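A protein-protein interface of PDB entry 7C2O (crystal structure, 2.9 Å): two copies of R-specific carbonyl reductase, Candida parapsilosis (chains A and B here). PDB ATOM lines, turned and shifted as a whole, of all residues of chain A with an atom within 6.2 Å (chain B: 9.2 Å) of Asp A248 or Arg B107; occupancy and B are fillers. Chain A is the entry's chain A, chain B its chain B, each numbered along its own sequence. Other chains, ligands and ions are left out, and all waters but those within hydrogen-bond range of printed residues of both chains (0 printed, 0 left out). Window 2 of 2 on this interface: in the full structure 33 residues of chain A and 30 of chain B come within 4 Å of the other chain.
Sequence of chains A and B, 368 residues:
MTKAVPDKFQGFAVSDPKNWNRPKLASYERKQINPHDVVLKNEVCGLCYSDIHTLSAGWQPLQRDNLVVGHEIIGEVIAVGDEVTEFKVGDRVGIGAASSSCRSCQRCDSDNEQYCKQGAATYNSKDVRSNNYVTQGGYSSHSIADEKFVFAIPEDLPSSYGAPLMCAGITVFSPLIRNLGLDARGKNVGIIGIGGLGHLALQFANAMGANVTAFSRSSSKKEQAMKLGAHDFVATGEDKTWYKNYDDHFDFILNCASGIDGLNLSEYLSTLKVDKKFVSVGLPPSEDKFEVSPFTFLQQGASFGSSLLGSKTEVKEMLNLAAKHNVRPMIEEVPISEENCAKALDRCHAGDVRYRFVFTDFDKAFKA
The side-chain carboxylate of Asp A248 lies within salt-bridge range of the guanidinium group of Arg B107, at 3.0 Å. The side-chain amide oxygen of Gln A300 lies within hydrogen-bond range of the guanidinium group of Arg B107 (3.4 Å).
The backbone carbonyl oxygen (O) of Ser A270 lies close to the side-chain amide oxygen (OE1) of Gln A300 (3.1 Å). OE1 of Gln A300 sits close to O of Leu A272, 2.8 Å away. The backbone NH (N) of Arg B107 sits close to the side-chain sulfur (SG) of Cys B105 (3.0 Å). The backbone NH of Asn B112 lies within hydrogen-bond range of the backbone carbonyl oxygen of Arg B107, 2.8 Å away. The side-chain amide oxygen (OD1) of Asn B112 is in hydrogen-bond range of the guanidinium group (NH2) of Arg B178. OH of Tyr B115 is in hydrogen-bond range of N of Leu B308 (2.9 Å).
Val A274 touches Arg B107 (CG2 to CD, 3.7 Å). OD1 of Asn B112 touches CG1 of Val A274, at 3.7 Å. Tyr B115 touches Val A274. NH1 of Arg B178 touches CG1 of Val A274, 3.8 Å away. Gln A299 touches Arg B107 (O to NH1, 3.7 Å). Gln A299 touches Tyr B115 (O to CD1, 3.1 Å).
Asp A248 touches just one residue of chain B: Arg B107. Arg B107 touches just these residues of chain A: Asp A248, Val A274, Gln A299 and Gln A300. No residue of chain B comes within 4 Å of Asp A247. Printed residues of chain B within 4 Å of Val A274: Arg B107, Asn B112, Tyr B115 and Arg B178. Printed residues of chain A within 4 Å of Asn B112: Val A274 (3.7 Å). Leu B308 touches none of the printed residues of chain A. Tyr A246 touches none of the printed residues of chain B. The nearest residue of chain B that does not touch Asp A248 is Gln B106 (4.1 Å). The nearest residue of chain A that does not touch Arg B107 is Leu A272 (4.05 Å). The nearest printed residue of chain B that does not touch Val A274 is Gln B114 (6.0 Å).
Of the 12 printed residues of chain A, 4 touch a printed residue of chain B. Printed residues of chain A that touch a printed residue of chain B: Asp A248, Val A274, Gln A299 and Gln A300. Hydrophobic or aromatic side chains of chain A that line the printed part of chain B: Val A274. Among the printed residues, Asp or Glu carboxylates within 4 Å of a Lys or Arg side-chain nitrogen of the other chain: Asp A248 with Arg B107 (3.0 Å).
No position is printed for both chains. Of the 8 pairs that touch across the chains among the printed residues, none has its exchanged pair printed and touching as well.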
ATOM      1  N   TYR A 246      -3.603 -18.037  34.620  1.00  0.00           N
ATOM      2  CA  TYR A 246      -4.630 -17.158  34.072  1.00  0.00           C
ATOM      3  C   TYR A 246      -4.019 -15.925  33.415  1.00  0.00           C
ATOM      4  O   TYR A 246      -4.635 -14.858  33.389  1.00  0.00           O
ATOM      5  CB  TYR A 246      -5.628 -16.751  35.156  1.00  0.00           C
ATOM      6  CG  TYR A 246      -6.545 -17.871  35.594  1.00  0.00           C
ATOM      7  CD1 TYR A 246      -7.851 -17.946  35.132  1.00  0.00           C
ATOM      8  CD2 TYR A 246      -6.100 -18.858  36.465  1.00  0.00           C
ATOM      9  CE1 TYR A 246      -8.692 -18.970  35.528  1.00  0.00           C
ATOM     10  CE2 TYR A 246      -6.930 -19.884  36.867  1.00  0.00           C
ATOM     11  CZ  TYR A 246      -8.227 -19.938  36.397  1.00  0.00           C
ATOM     12  OH  TYR A 246      -9.060 -20.961  36.798  1.00  0.00           O
ATOM     13  N   ASP A 247      -2.809 -16.058  32.879  1.00  0.00           N
ATOM     14  CA  ASP A 247      -2.143 -14.925  32.253  1.00  0.00           C
ATOM     15  C   ASP A 247      -2.929 -14.459  31.037  1.00  0.00           C
ATOM     16  O   ASP A 247      -3.113 -15.219  30.080  1.00  0.00           O
ATOM     17  CB  ASP A 247      -0.719 -15.305  31.855  1.00  0.00           C
ATOM     18  CG  ASP A 247       0.257 -14.160  32.033  1.00  0.00           C
ATOM     19  OD1 ASP A 247       1.070 -14.213  32.979  1.00  0.00           O
ATOM     20  OD2 ASP A 247       0.204 -13.203  31.232  1.00  0.00           O
ATOM     21  N   ASP A 248      -3.400 -13.211  31.086  1.00  0.00           N
ATOM     22  CA  ASP A 248      -4.132 -12.584  29.985  1.00  0.00           C
ATOM     23  C   ASP A 248      -5.382 -13.392  29.627  1.00  0.00           C
ATOM     24  O   ASP A 248      -5.531 -13.906  28.516  1.00  0.00           O
ATOM     25  CB  ASP A 248      -3.220 -12.392  28.769  1.00  0.00           C
ATOM     26  CG  ASP A 248      -3.846 -11.521  27.699  1.00  0.00           C
ATOM     27  OD1 ASP A 248      -3.884 -10.282  27.880  1.00  0.00           O
ATOM     28  OD2 ASP A 248      -4.304 -12.080  26.678  1.00  0.00           O
ATOM     29  N   HIS A 249      -6.290 -13.485  30.590  1.00  0.00           N
ATOM     30  CA  HIS A 249      -7.478 -14.318  30.426  1.00  0.00           C
ATOM     31  C   HIS A 249      -8.779 -13.601  30.757  1.00  0.00           C
ATOM     32  O   HIS A 249      -9.774 -13.795  30.054  1.00  0.00           O
ATOM     33  CB  HIS A 249      -7.351 -15.582  31.297  1.00  0.00           C
ATOM     34  CG  HIS A 249      -8.615 -16.380  31.390  1.00  0.00           C
ATOM     35  ND1 HIS A 249      -8.965 -17.332  30.457  1.00  0.00           N
ATOM     36  CD2 HIS A 249      -9.616 -16.362  32.303  1.00  0.00           C
ATOM     37  CE1 HIS A 249     -10.125 -17.869  30.793  1.00  0.00           C
ATOM     38  NE2 HIS A 249     -10.542 -17.297  31.908  1.00  0.00           N
ATOM     39  N   PHE A 250      -8.804 -12.787  31.805  1.00  0.00           N
ATOM     40  CA  PHE A 250     -10.050 -12.213  32.290  1.00  0.00           C
ATOM     41  C   PHE A 250     -10.403 -10.940  31.537  1.00  0.00           C
ATOM     42  O   PHE A 250      -9.547 -10.084  31.297  1.00  0.00           O
ATOM     43  CB  PHE A 250      -9.960 -11.922  33.787  1.00  0.00           C
ATOM     44  CG  PHE A 250     -10.136 -13.137  34.642  1.00  0.00           C
ATOM     45  CD1 PHE A 250     -11.401 -13.631  34.909  1.00  0.00           C
ATOM     46  CD2 PHE A 250      -9.038 -13.793  35.167  1.00  0.00           C
ATOM     47  CE1 PHE A 250     -11.566 -14.754  35.690  1.00  0.00           C
ATOM     48  CE2 PHE A 250      -9.198 -14.915  35.948  1.00  0.00           C
ATOM     49  CZ  PHE A 250     -10.463 -15.397  36.211  1.00  0.00           C
ATOM     50  N   SER A 270      -2.938  -9.321  37.640  1.00  0.00           N
ATOM     51  CA  SER A 270      -2.025 -10.023  36.743  1.00  0.00           C
ATOM     52  C   SER A 270      -2.773 -10.813  35.678  1.00  0.00           C
ATOM     53  O   SER A 270      -2.238 -11.044  34.587  1.00  0.00           O
ATOM     54  CB  SER A 270      -1.120 -10.959  37.551  1.00  0.00           C
ATOM     55  OG  SER A 270      -0.312 -10.229  38.459  1.00  0.00           O
ATOM     56  N   THR A 271      -4.005 -11.224  35.971  1.00  0.00           N
ATOM     57  CA  THR A 271      -4.777 -12.103  35.105  1.00  0.00           C
ATOM     58  C   THR A 271      -5.697 -11.354  34.153  1.00  0.00           C
ATOM     59  O   THR A 271      -6.346 -11.987  33.313  1.00  0.00           O
ATOM     60  CB  THR A 271      -5.603 -13.068  35.953  1.00  0.00           C
ATOM     61  OG1 THR A 271      -6.687 -12.353  36.561  1.00  0.00           O
ATOM     62  CG2 THR A 271      -4.738 -13.689  37.040  1.00  0.00           C
ATOM     63  N   LEU A 272      -5.775 -10.033  34.262  1.00  0.00           N
ATOM     64  CA  LEU A 272      -6.635  -9.260  33.383  1.00  0.00           C
ATOM     65  C   LEU A 272      -5.967  -9.036  32.034  1.00  0.00           C
ATOM     66  O   LEU A 272      -4.738  -9.042  31.914  1.00  0.00           O
ATOM     67  CB  LEU A 272      -6.985  -7.916  34.020  1.00  0.00           C
ATOM     68  CG  LEU A 272      -8.159  -7.922  34.996  1.00  0.00           C
ATOM     69  CD1 LEU A 272      -8.284  -6.572  35.677  1.00  0.00           C
ATOM     70  CD2 LEU A 272      -9.447  -8.287  34.279  1.00  0.00           C
ATOM     71  N   LYS A 273      -6.793  -8.851  31.011  1.00  0.00           N
ATOM     72  CA  LYS A 273      -6.295  -8.438  29.711  1.00  0.00           C
ATOM     73  C   LYS A 273      -6.009  -6.939  29.731  1.00  0.00           C
ATOM     74  O   LYS A 273      -6.261  -6.242  30.719  1.00  0.00           O
ATOM     75  CB  LYS A 273      -7.291  -8.808  28.617  1.00  0.00           C
ATOM     76  CG  LYS A 273      -7.411 -10.301  28.374  1.00  0.00           C
ATOM     77  CD  LYS A 273      -8.353 -10.596  27.222  1.00  0.00           C
ATOM     78  CE  LYS A 273      -9.392 -11.626  27.616  1.00  0.00           C
ATOM     79  NZ  LYS A 273     -10.377 -11.870  26.528  1.00  0.00           N
ATOM     80  N   VAL A 274      -5.481  -6.427  28.620  1.00  0.00           N
ATOM     81  CA  VAL A 274      -5.026  -5.043  28.584  1.00  0.00           C
ATOM     82  C   VAL A 274      -6.223  -4.104  28.650  1.00  0.00           C
ATOM     83  O   VAL A 274      -7.235  -4.312  27.968  1.00  0.00           O
ATOM     84  CB  VAL A 274      -4.180  -4.789  27.330  1.00  0.00           C
ATOM     85  CG1 VAL A 274      -3.503  -3.435  27.426  1.00  0.00           C
ATOM     86  CG2 VAL A 274      -3.143  -5.890  27.163  1.00  0.00           C
ATOM     87  N   GLN A 299       2.060  -2.921  33.548  1.00  0.00           N
ATOM     88  CA  GLN A 299       2.218  -4.109  32.715  1.00  0.00           C
ATOM     89  C   GLN A 299       0.924  -4.467  32.001  1.00  0.00           C
ATOM     90  O   GLN A 299       0.948  -4.861  30.830  1.00  0.00           O
ATOM     91  CB  GLN A 299       2.692  -5.284  33.554  1.00  0.00           C
ATOM     92  CG  GLN A 299       4.096  -5.169  34.147  1.00  0.00           C
ATOM     93  CD  GLN A 299       4.668  -6.530  34.524  1.00  0.00           C
ATOM     94  OE1 GLN A 299       5.872  -6.779  34.381  1.00  0.00           O
ATOM     95  NE2 GLN A 299       3.800  -7.428  34.978  1.00  0.00           N
ATOM     96  N   GLN A 300      -0.215  -4.373  32.688  1.00  0.00           N
ATOM     97  CA  GLN A 300      -1.485  -4.717  32.067  1.00  0.00           C
ATOM     98  C   GLN A 300      -2.249  -3.503  31.566  1.00  0.00           C
ATOM     99  O   GLN A 300      -3.157  -3.662  30.745  1.00  0.00           O
ATOM    100  CB  GLN A 300      -2.371  -5.490  33.054  1.00  0.00           C
ATOM    101  CG  GLN A 300      -1.635  -6.538  33.864  1.00  0.00           C
ATOM    102  CD  GLN A 300      -1.240  -7.744  33.032  1.00  0.00           C
ATOM    103  OE1 GLN A 300      -2.079  -8.577  32.684  1.00  0.00           O
ATOM    104  NE2 GLN A 300       0.045  -7.840  32.704  1.00  0.00           N
ATOM    105  N   SER B 101       9.486  -7.825  20.564  1.00  0.00           N
ATOM    106  CA  SER B 101       8.234  -8.387  21.053  1.00  0.00           C
ATOM    107  C   SER B 101       8.246  -9.895  20.833  1.00  0.00           C
ATOM    108  O   SER B 101       9.185 -10.455  20.257  1.00  0.00           O
ATOM    109  CB  SER B 101       7.031  -7.738  20.364  1.00  0.00           C
ATOM    110  OG  SER B 101       5.813  -8.170  20.944  1.00  0.00           O
ATOM    111  N   CYS B 102       7.177 -10.551  21.294  1.00  0.00           N
ATOM    112  CA  CYS B 102       7.105 -12.010  21.244  1.00  0.00           C
ATOM    113  C   CYS B 102       6.848 -12.511  19.828  1.00  0.00           C
ATOM    114  O   CYS B 102       7.397 -13.541  19.420  1.00  0.00           O
ATOM    115  CB  CYS B 102       6.009 -12.502  22.186  1.00  0.00           C
ATOM    116  SG  CYS B 102       6.185 -14.191  22.765  1.00  0.00           S
ATOM    117  N   ARG B 103       6.005 -11.804  19.077  1.00  0.00           N
ATOM    118  CA  ARG B 103       5.559 -12.169  17.735  1.00  0.00           C
ATOM    119  C   ARG B 103       4.811 -13.498  17.701  1.00  0.00           C
ATOM    120  O   ARG B 103       4.607 -14.061  16.620  1.00  0.00           O
ATOM    121  CB  ARG B 103       6.727 -12.195  16.739  1.00  0.00           C
ATOM    122  CG  ARG B 103       7.040 -10.843  16.105  1.00  0.00           C
ATOM    123  CD  ARG B 103       7.835 -11.018  14.826  1.00  0.00           C
ATOM    124  NE  ARG B 103       8.170  -9.744  14.197  1.00  0.00           N
ATOM    125  CZ  ARG B 103       7.394  -9.117  13.318  1.00  0.00           C
ATOM    126  NH1 ARG B 103       6.230  -9.645  12.960  1.00  0.00           N
ATOM    127  NH2 ARG B 103       7.779  -7.962  12.795  1.00  0.00           N
ATOM    128  N   SER B 104       4.388 -14.009  18.855  1.00  0.00           N
ATOM    129  CA  SER B 104       3.662 -15.272  18.904  1.00  0.00           C
ATOM    130  C   SER B 104       2.666 -15.352  20.051  1.00  0.00           C
ATOM    131  O   SER B 104       2.018 -16.392  20.199  1.00  0.00           O
ATOM    132  CB  SER B 104       4.651 -16.448  18.998  1.00  0.00           C
ATOM    133  OG  SER B 104       5.565 -16.447  17.916  1.00  0.00           O
ATOM    134  N   CYS B 105       2.521 -14.307  20.864  1.00  0.00           N
ATOM    135  CA  CYS B 105       1.591 -14.318  21.988  1.00  0.00           C
ATOM    136  C   CYS B 105       0.174 -14.009  21.523  1.00  0.00           C
ATOM    137  O   CYS B 105      -0.230 -14.403  20.424  1.00  0.00           O
ATOM    138  CB  CYS B 105       2.027 -13.303  23.051  1.00  0.00           C
ATOM    139  SG  CYS B 105       1.807 -11.569  22.572  1.00  0.00           S
ATOM    140  N   GLN B 106      -0.590 -13.315  22.366  1.00  0.00           N
ATOM    141  CA  GLN B 106      -1.875 -12.759  21.971  1.00  0.00           C
ATOM    142  C   GLN B 106      -1.872 -11.240  21.924  1.00  0.00           C
ATOM    143  O   GLN B 106      -2.678 -10.660  21.191  1.00  0.00           O
ATOM    144  CB  GLN B 106      -2.981 -13.229  22.929  1.00  0.00           C
ATOM    145  N   ARG B 107      -0.982 -10.592  22.680  1.00  0.00           N
ATOM    146  CA  ARG B 107      -0.869  -9.138  22.627  1.00  0.00           C
ATOM    147  C   ARG B 107      -0.357  -8.676  21.269  1.00  0.00           C
ATOM    148  O   ARG B 107      -0.839  -7.676  20.724  1.00  0.00           O
ATOM    149  CB  ARG B 107       0.064  -8.651  23.736  1.00  0.00           C
ATOM    150  CG  ARG B 107      -0.089  -9.375  25.067  1.00  0.00           C
ATOM    151  CD  ARG B 107      -0.670  -8.448  26.122  1.00  0.00           C
ATOM    152  NE  ARG B 107      -1.198  -9.174  27.275  1.00  0.00           N
ATOM    153  CZ  ARG B 107      -0.993  -8.826  28.543  1.00  0.00           C
ATOM    154  NH1 ARG B 107      -0.268  -7.753  28.834  1.00  0.00           N
ATOM    155  NH2 ARG B 107      -1.515  -9.550  29.523  1.00  0.00           N
ATOM    156  N   CYS B 108       0.620  -9.390  20.710  1.00  0.00           N
ATOM    157  CA  CYS B 108       1.188  -8.997  19.426  1.00  0.00           C
ATOM    158  C   CYS B 108       0.173  -9.124  18.299  1.00  0.00           C
ATOM    159  O   CYS B 108       0.210  -8.339  17.344  1.00  0.00           O
ATOM    160  CB  CYS B 108       2.430  -9.837  19.132  1.00  0.00           C
ATOM    161  SG  CYS B 108       3.772  -9.605  20.326  1.00  0.00           S
ATOM    162  N   ASP B 109      -0.742 -10.087  18.393  1.00  0.00           N
ATOM    163  CA  ASP B 109      -1.739 -10.289  17.352  1.00  0.00           C
ATOM    164  C   ASP B 109      -2.969  -9.409  17.521  1.00  0.00           C
ATOM    165  O   ASP B 109      -3.742  -9.262  16.566  1.00  0.00           O
ATOM    166  CB  ASP B 109      -2.171 -11.757  17.314  1.00  0.00           C
ATOM    167  CG  ASP B 109      -1.079 -12.671  16.801  1.00  0.00           C
ATOM    168  OD1 ASP B 109      -0.414 -12.303  15.809  1.00  0.00           O
ATOM    169  OD2 ASP B 109      -0.883 -13.756  17.392  1.00  0.00           O
ATOM    170  N   SER B 110      -3.170  -8.821  18.699  1.00  0.00           N
ATOM    171  CA  SER B 110      -4.366  -8.040  18.990  1.00  0.00           C
ATOM    172  C   SER B 110      -4.039  -6.574  19.252  1.00  0.00           C
ATOM    173  O   SER B 110      -4.704  -5.920  20.060  1.00  0.00           O
ATOM    174  CB  SER B 110      -5.125  -8.638  20.175  1.00  0.00           C
ATOM    175  N   ASP B 111      -3.013  -6.048  18.576  1.00  0.00           N
ATOM    176  CA  ASP B 111      -2.651  -4.630  18.650  1.00  0.00           C
ATOM    177  C   ASP B 111      -2.292  -4.212  20.077  1.00  0.00           C
ATOM    178  O   ASP B 111      -2.808  -3.227  20.609  1.00  0.00           O
ATOM    179  CB  ASP B 111      -3.772  -3.748  18.094  1.00  0.00           C
ATOM    180  CG  ASP B 111      -3.400  -3.088  16.787  1.00  0.00           C
ATOM    181  OD1 ASP B 111      -2.373  -3.477  16.191  1.00  0.00           O
ATOM    182  OD2 ASP B 111      -4.139  -2.178  16.356  1.00  0.00           O
ATOM    183  N   ASN B 112      -1.386  -4.971  20.695  1.00  0.00           N
ATOM    184  CA  ASN B 112      -0.941  -4.672  22.053  1.00  0.00           C
ATOM    185  C   ASN B 112       0.483  -5.174  22.261  1.00  0.00           C
ATOM    186  O   ASN B 112       0.846  -5.621  23.354  1.00  0.00           O
ATOM    187  CB  ASN B 112      -1.886  -5.274  23.097  1.00  0.00           C
ATOM    188  CG  ASN B 112      -3.018  -4.332  23.478  1.00  0.00           C
ATOM    189  OD1 ASN B 112      -2.794  -3.159  23.774  1.00  0.00           O
ATOM    190  ND2 ASN B 112      -4.243  -4.846  23.465  1.00  0.00           N
ATOM    191  N   GLU B 113       1.309  -5.096  21.212  1.00  0.00           N
ATOM    192  CA  GLU B 113       2.676  -5.602  21.288  1.00  0.00           C
ATOM    193  C   GLU B 113       3.522  -4.850  22.312  1.00  0.00           C
ATOM    194  O   GLU B 113       4.496  -5.411  22.825  1.00  0.00           O
ATOM    195  CB  GLU B 113       3.339  -5.539  19.907  1.00  0.00           C
ATOM    196  CG  GLU B 113       3.466  -4.134  19.329  1.00  0.00           C
ATOM    197  CD  GLU B 113       2.211  -3.686  18.600  1.00  0.00           C
ATOM    198  OE1 GLU B 113       1.260  -4.491  18.506  1.00  0.00           O
ATOM    199  OE2 GLU B 113       2.173  -2.527  18.129  1.00  0.00           O
ATOM    200  N   GLN B 114       3.175  -3.600  22.627  1.00  0.00           N
ATOM    201  CA  GLN B 114       3.927  -2.852  23.629  1.00  0.00           C
ATOM    202  C   GLN B 114       3.689  -3.364  25.045  1.00  0.00           C
ATOM    203  O   GLN B 114       4.451  -3.006  25.949  1.00  0.00           O
ATOM    204  CB  GLN B 114       3.575  -1.365  23.551  1.00  0.00           C
ATOM    205  CG  GLN B 114       2.220  -1.007  24.145  1.00  0.00           C
ATOM    206  CD  GLN B 114       1.083  -1.199  23.160  1.00  0.00           C
ATOM    207  OE1 GLN B 114       1.222  -1.906  22.159  1.00  0.00           O
ATOM    208  NE2 GLN B 114      -0.051  -0.561  23.436  1.00  0.00           N
ATOM    209  N   TYR B 115       2.659  -4.183  25.256  1.00  0.00           N
ATOM    210  CA  TYR B 115       2.343  -4.747  26.562  1.00  0.00           C
ATOM    211  C   TYR B 115       2.761  -6.209  26.681  1.00  0.00           C
ATOM    212  O   TYR B 115       2.365  -6.882  27.640  1.00  0.00           O
ATOM    213  CB  TYR B 115       0.845  -4.611  26.847  1.00  0.00           C
ATOM    214  CG  TYR B 115       0.378  -3.228  27.272  1.00  0.00           C
ATOM    215  CD1 TYR B 115       0.615  -2.753  28.557  1.00  0.00           C
ATOM    216  CD2 TYR B 115      -0.324  -2.410  26.392  1.00  0.00           C
ATOM    217  CE1 TYR B 115       0.179  -1.500  28.951  1.00  0.00           C
ATOM    218  CE2 TYR B 115      -0.766  -1.156  26.776  1.00  0.00           C
ATOM    219  CZ  TYR B 115      -0.512  -0.703  28.057  1.00  0.00           C
ATOM    220  OH  TYR B 115      -0.952   0.548  28.441  1.00  0.00           O
ATOM    221  N   CYS B 116       3.546  -6.712  25.732  1.00  0.00           N
ATOM    222  CA  CYS B 116       3.956  -8.109  25.737  1.00  0.00           C
ATOM    223  C   CYS B 116       4.945  -8.374  26.866  1.00  0.00           C
ATOM    224  O   CYS B 116       5.931  -7.646  27.025  1.00  0.00           O
ATOM    225  CB  CYS B 116       4.568  -8.470  24.382  1.00  0.00           C
ATOM    226  SG  CYS B 116       5.729  -9.857  24.374  1.00  0.00           S
ATOM    227  N   LYS B 117       4.680  -9.428  27.649  1.00  0.00           N
ATOM    228  CA  LYS B 117       5.494  -9.719  28.826  1.00  0.00           C
ATOM    229  C   LYS B 117       6.916 -10.116  28.452  1.00  0.00           C
ATOM    230  O   LYS B 117       7.840  -9.929  29.251  1.00  0.00           O
ATOM    231  CB  LYS B 117       4.841 -10.824  29.661  1.00  0.00           C
ATOM    232  CG  LYS B 117       5.291 -10.859  31.117  1.00  0.00           C
ATOM    233  CD  LYS B 117       4.589 -11.967  31.894  1.00  0.00           C
ATOM    234  N   GLN B 118       7.113 -10.667  27.256  1.00  0.00           N
ATOM    235  CA  GLN B 118       8.433 -11.054  26.783  1.00  0.00           C
ATOM    236  C   GLN B 118       9.057  -9.999  25.874  1.00  0.00           C
ATOM    237  O   GLN B 118       9.976 -10.312  25.111  1.00  0.00           O
ATOM    238  CB  GLN B 118       8.358 -12.400  26.061  1.00  0.00           C
ATOM    239  CG  GLN B 118       7.973 -13.565  26.961  1.00  0.00           C
ATOM    240  CD  GLN B 118       7.943 -14.889  26.219  1.00  0.00           C
ATOM    241  OE1 GLN B 118       6.891 -15.330  25.754  1.00  0.00           O
ATOM    242  NE2 GLN B 118       9.103 -15.528  26.101  1.00  0.00           N
ATOM    243  N   GLY B 119       8.576  -8.754  25.939  1.00  0.00           N
ATOM    244  CA  GLY B 119       9.110  -7.707  25.096  1.00  0.00           C
ATOM    245  C   GLY B 119      10.388  -7.102  25.646  1.00  0.00           C
ATOM    246  O   GLY B 119      10.773  -7.317  26.794  1.00  0.00           O
ATOM    247  N   LYS B 148       7.800  -4.264  13.919  1.00  0.00           N
ATOM    248  CA  LYS B 148       6.555  -3.745  14.473  1.00  0.00           C
ATOM    249  C   LYS B 148       6.762  -2.592  15.444  1.00  0.00           C
ATOM    250  O   LYS B 148       5.772  -2.024  15.921  1.00  0.00           O
ATOM    251  CB  LYS B 148       5.773  -4.859  15.157  1.00  0.00           C
ATOM    252  CG  LYS B 148       4.290  -4.837  14.831  1.00  0.00           C
ATOM    253  CD  LYS B 148       3.506  -5.753  15.763  1.00  0.00           C
ATOM    254  CE  LYS B 148       4.152  -7.129  15.838  1.00  0.00           C
ATOM    255  NZ  LYS B 148       3.829  -7.966  14.645  1.00  0.00           N
ATOM    256  N   PHE B 149       8.010  -2.228  15.732  1.00  0.00           N
ATOM    257  CA  PHE B 149       8.329  -1.047  16.522  1.00  0.00           C
ATOM    258  C   PHE B 149       9.053   0.006  15.700  1.00  0.00           C
ATOM    259  O   PHE B 149       9.489   1.025  16.245  1.00  0.00           O
ATOM    260  CB  PHE B 149       9.153  -1.442  17.745  1.00  0.00           C
ATOM    261  CG  PHE B 149       8.435  -2.384  18.659  1.00  0.00           C
ATOM    262  CD1 PHE B 149       7.597  -1.903  19.651  1.00  0.00           C
ATOM    263  CD2 PHE B 149       8.573  -3.751  18.511  1.00  0.00           C
ATOM    264  CE1 PHE B 149       6.923  -2.768  20.486  1.00  0.00           C
ATOM    265  CE2 PHE B 149       7.904  -4.618  19.343  1.00  0.00           C
ATOM    266  CZ  PHE B 149       7.077  -4.128  20.331  1.00  0.00           C
ATOM    267  N   ARG B 178      -8.106   5.521  23.325  1.00  0.00           N
ATOM    268  CA  ARG B 178      -8.716   4.346  23.935  1.00  0.00           C
ATOM    269  C   ARG B 178      -9.834   4.712  24.898  1.00  0.00           C
ATOM    270  O   ARG B 178     -10.800   3.954  25.030  1.00  0.00           O
ATOM    271  CB  ARG B 178      -7.655   3.520  24.660  1.00  0.00           C
ATOM    272  CG  ARG B 178      -6.722   2.765  23.729  1.00  0.00           C
ATOM    273  CD  ARG B 178      -5.841   1.793  24.493  1.00  0.00           C
ATOM    274  NE  ARG B 178      -5.005   1.009  23.590  1.00  0.00           N
ATOM    275  CZ  ARG B 178      -4.347  -0.090  23.945  1.00  0.00           C
ATOM    276  NH1 ARG B 178      -4.429  -0.540  25.191  1.00  0.00           N
ATOM    277  NH2 ARG B 178      -3.606  -0.738  23.054  1.00  0.00           N
ATOM    278  N   LEU B 308       1.019   2.536  29.078  1.00  0.00           N
ATOM    279  CA  LEU B 308       2.398   2.506  28.609  1.00  0.00           C
ATOM    280  C   LEU B 308       2.406   2.516  27.088  1.00  0.00           C
ATOM    281  O   LEU B 308       1.788   1.650  26.460  1.00  0.00           O
ATOM    282  CB  LEU B 308       3.135   1.275  29.140  1.00  0.00           C
ATOM    283  CG  LEU B 308       4.549   1.075  28.586  1.00  0.00           C
ATOM    284  CD1 LEU B 308       5.556   1.939  29.341  1.00  0.00           C
ATOM    285  CD2 LEU B 308       4.961  -0.393  28.610  1.00  0.00           C
ATOM    286  N   SER B 311       0.089   1.351  20.500  1.00  0.00           N
ATOM    287  CA  SER B 311       0.193   0.335  19.462  1.00  0.00           C
ATOM    288  C   SER B 311       0.653   0.960  18.150  1.00  0.00           C
ATOM    289  O   SER B 311       0.533   2.167  17.932  1.00  0.00           O
ATOM    290  CB  SER B 311      -1.145  -0.379  19.261  1.00  0.00           C
ATOM    291  OG  SER B 311      -2.006   0.377  18.428  1.00  0.00           O
ATOM    292  N   LYS B 312       1.193   0.111  17.269  1.00  0.00           N
ATOM    293  CA  LYS B 312       1.691   0.596  15.985  1.00  0.00           C
ATOM    294  C   LYS B 312       0.575   1.224  15.157  1.00  0.00           C
ATOM    295  O   LYS B 312       0.786   2.242  14.485  1.00  0.00           O
ATOM    296  CB  LYS B 312       2.355  -0.547  15.215  1.00  0.00           C
ATOM    297  CG  LYS B 312       2.643  -0.229  13.751  1.00  0.00           C
ATOM    298  CD  LYS B 312       4.054  -0.633  13.352  1.00  0.00           C
ATOM    299  CE  LYS B 312       4.248  -0.552  11.847  1.00  0.00           C
ATOM    300  NZ  LYS B 312       5.615  -0.981  11.430  1.00  0.00           N
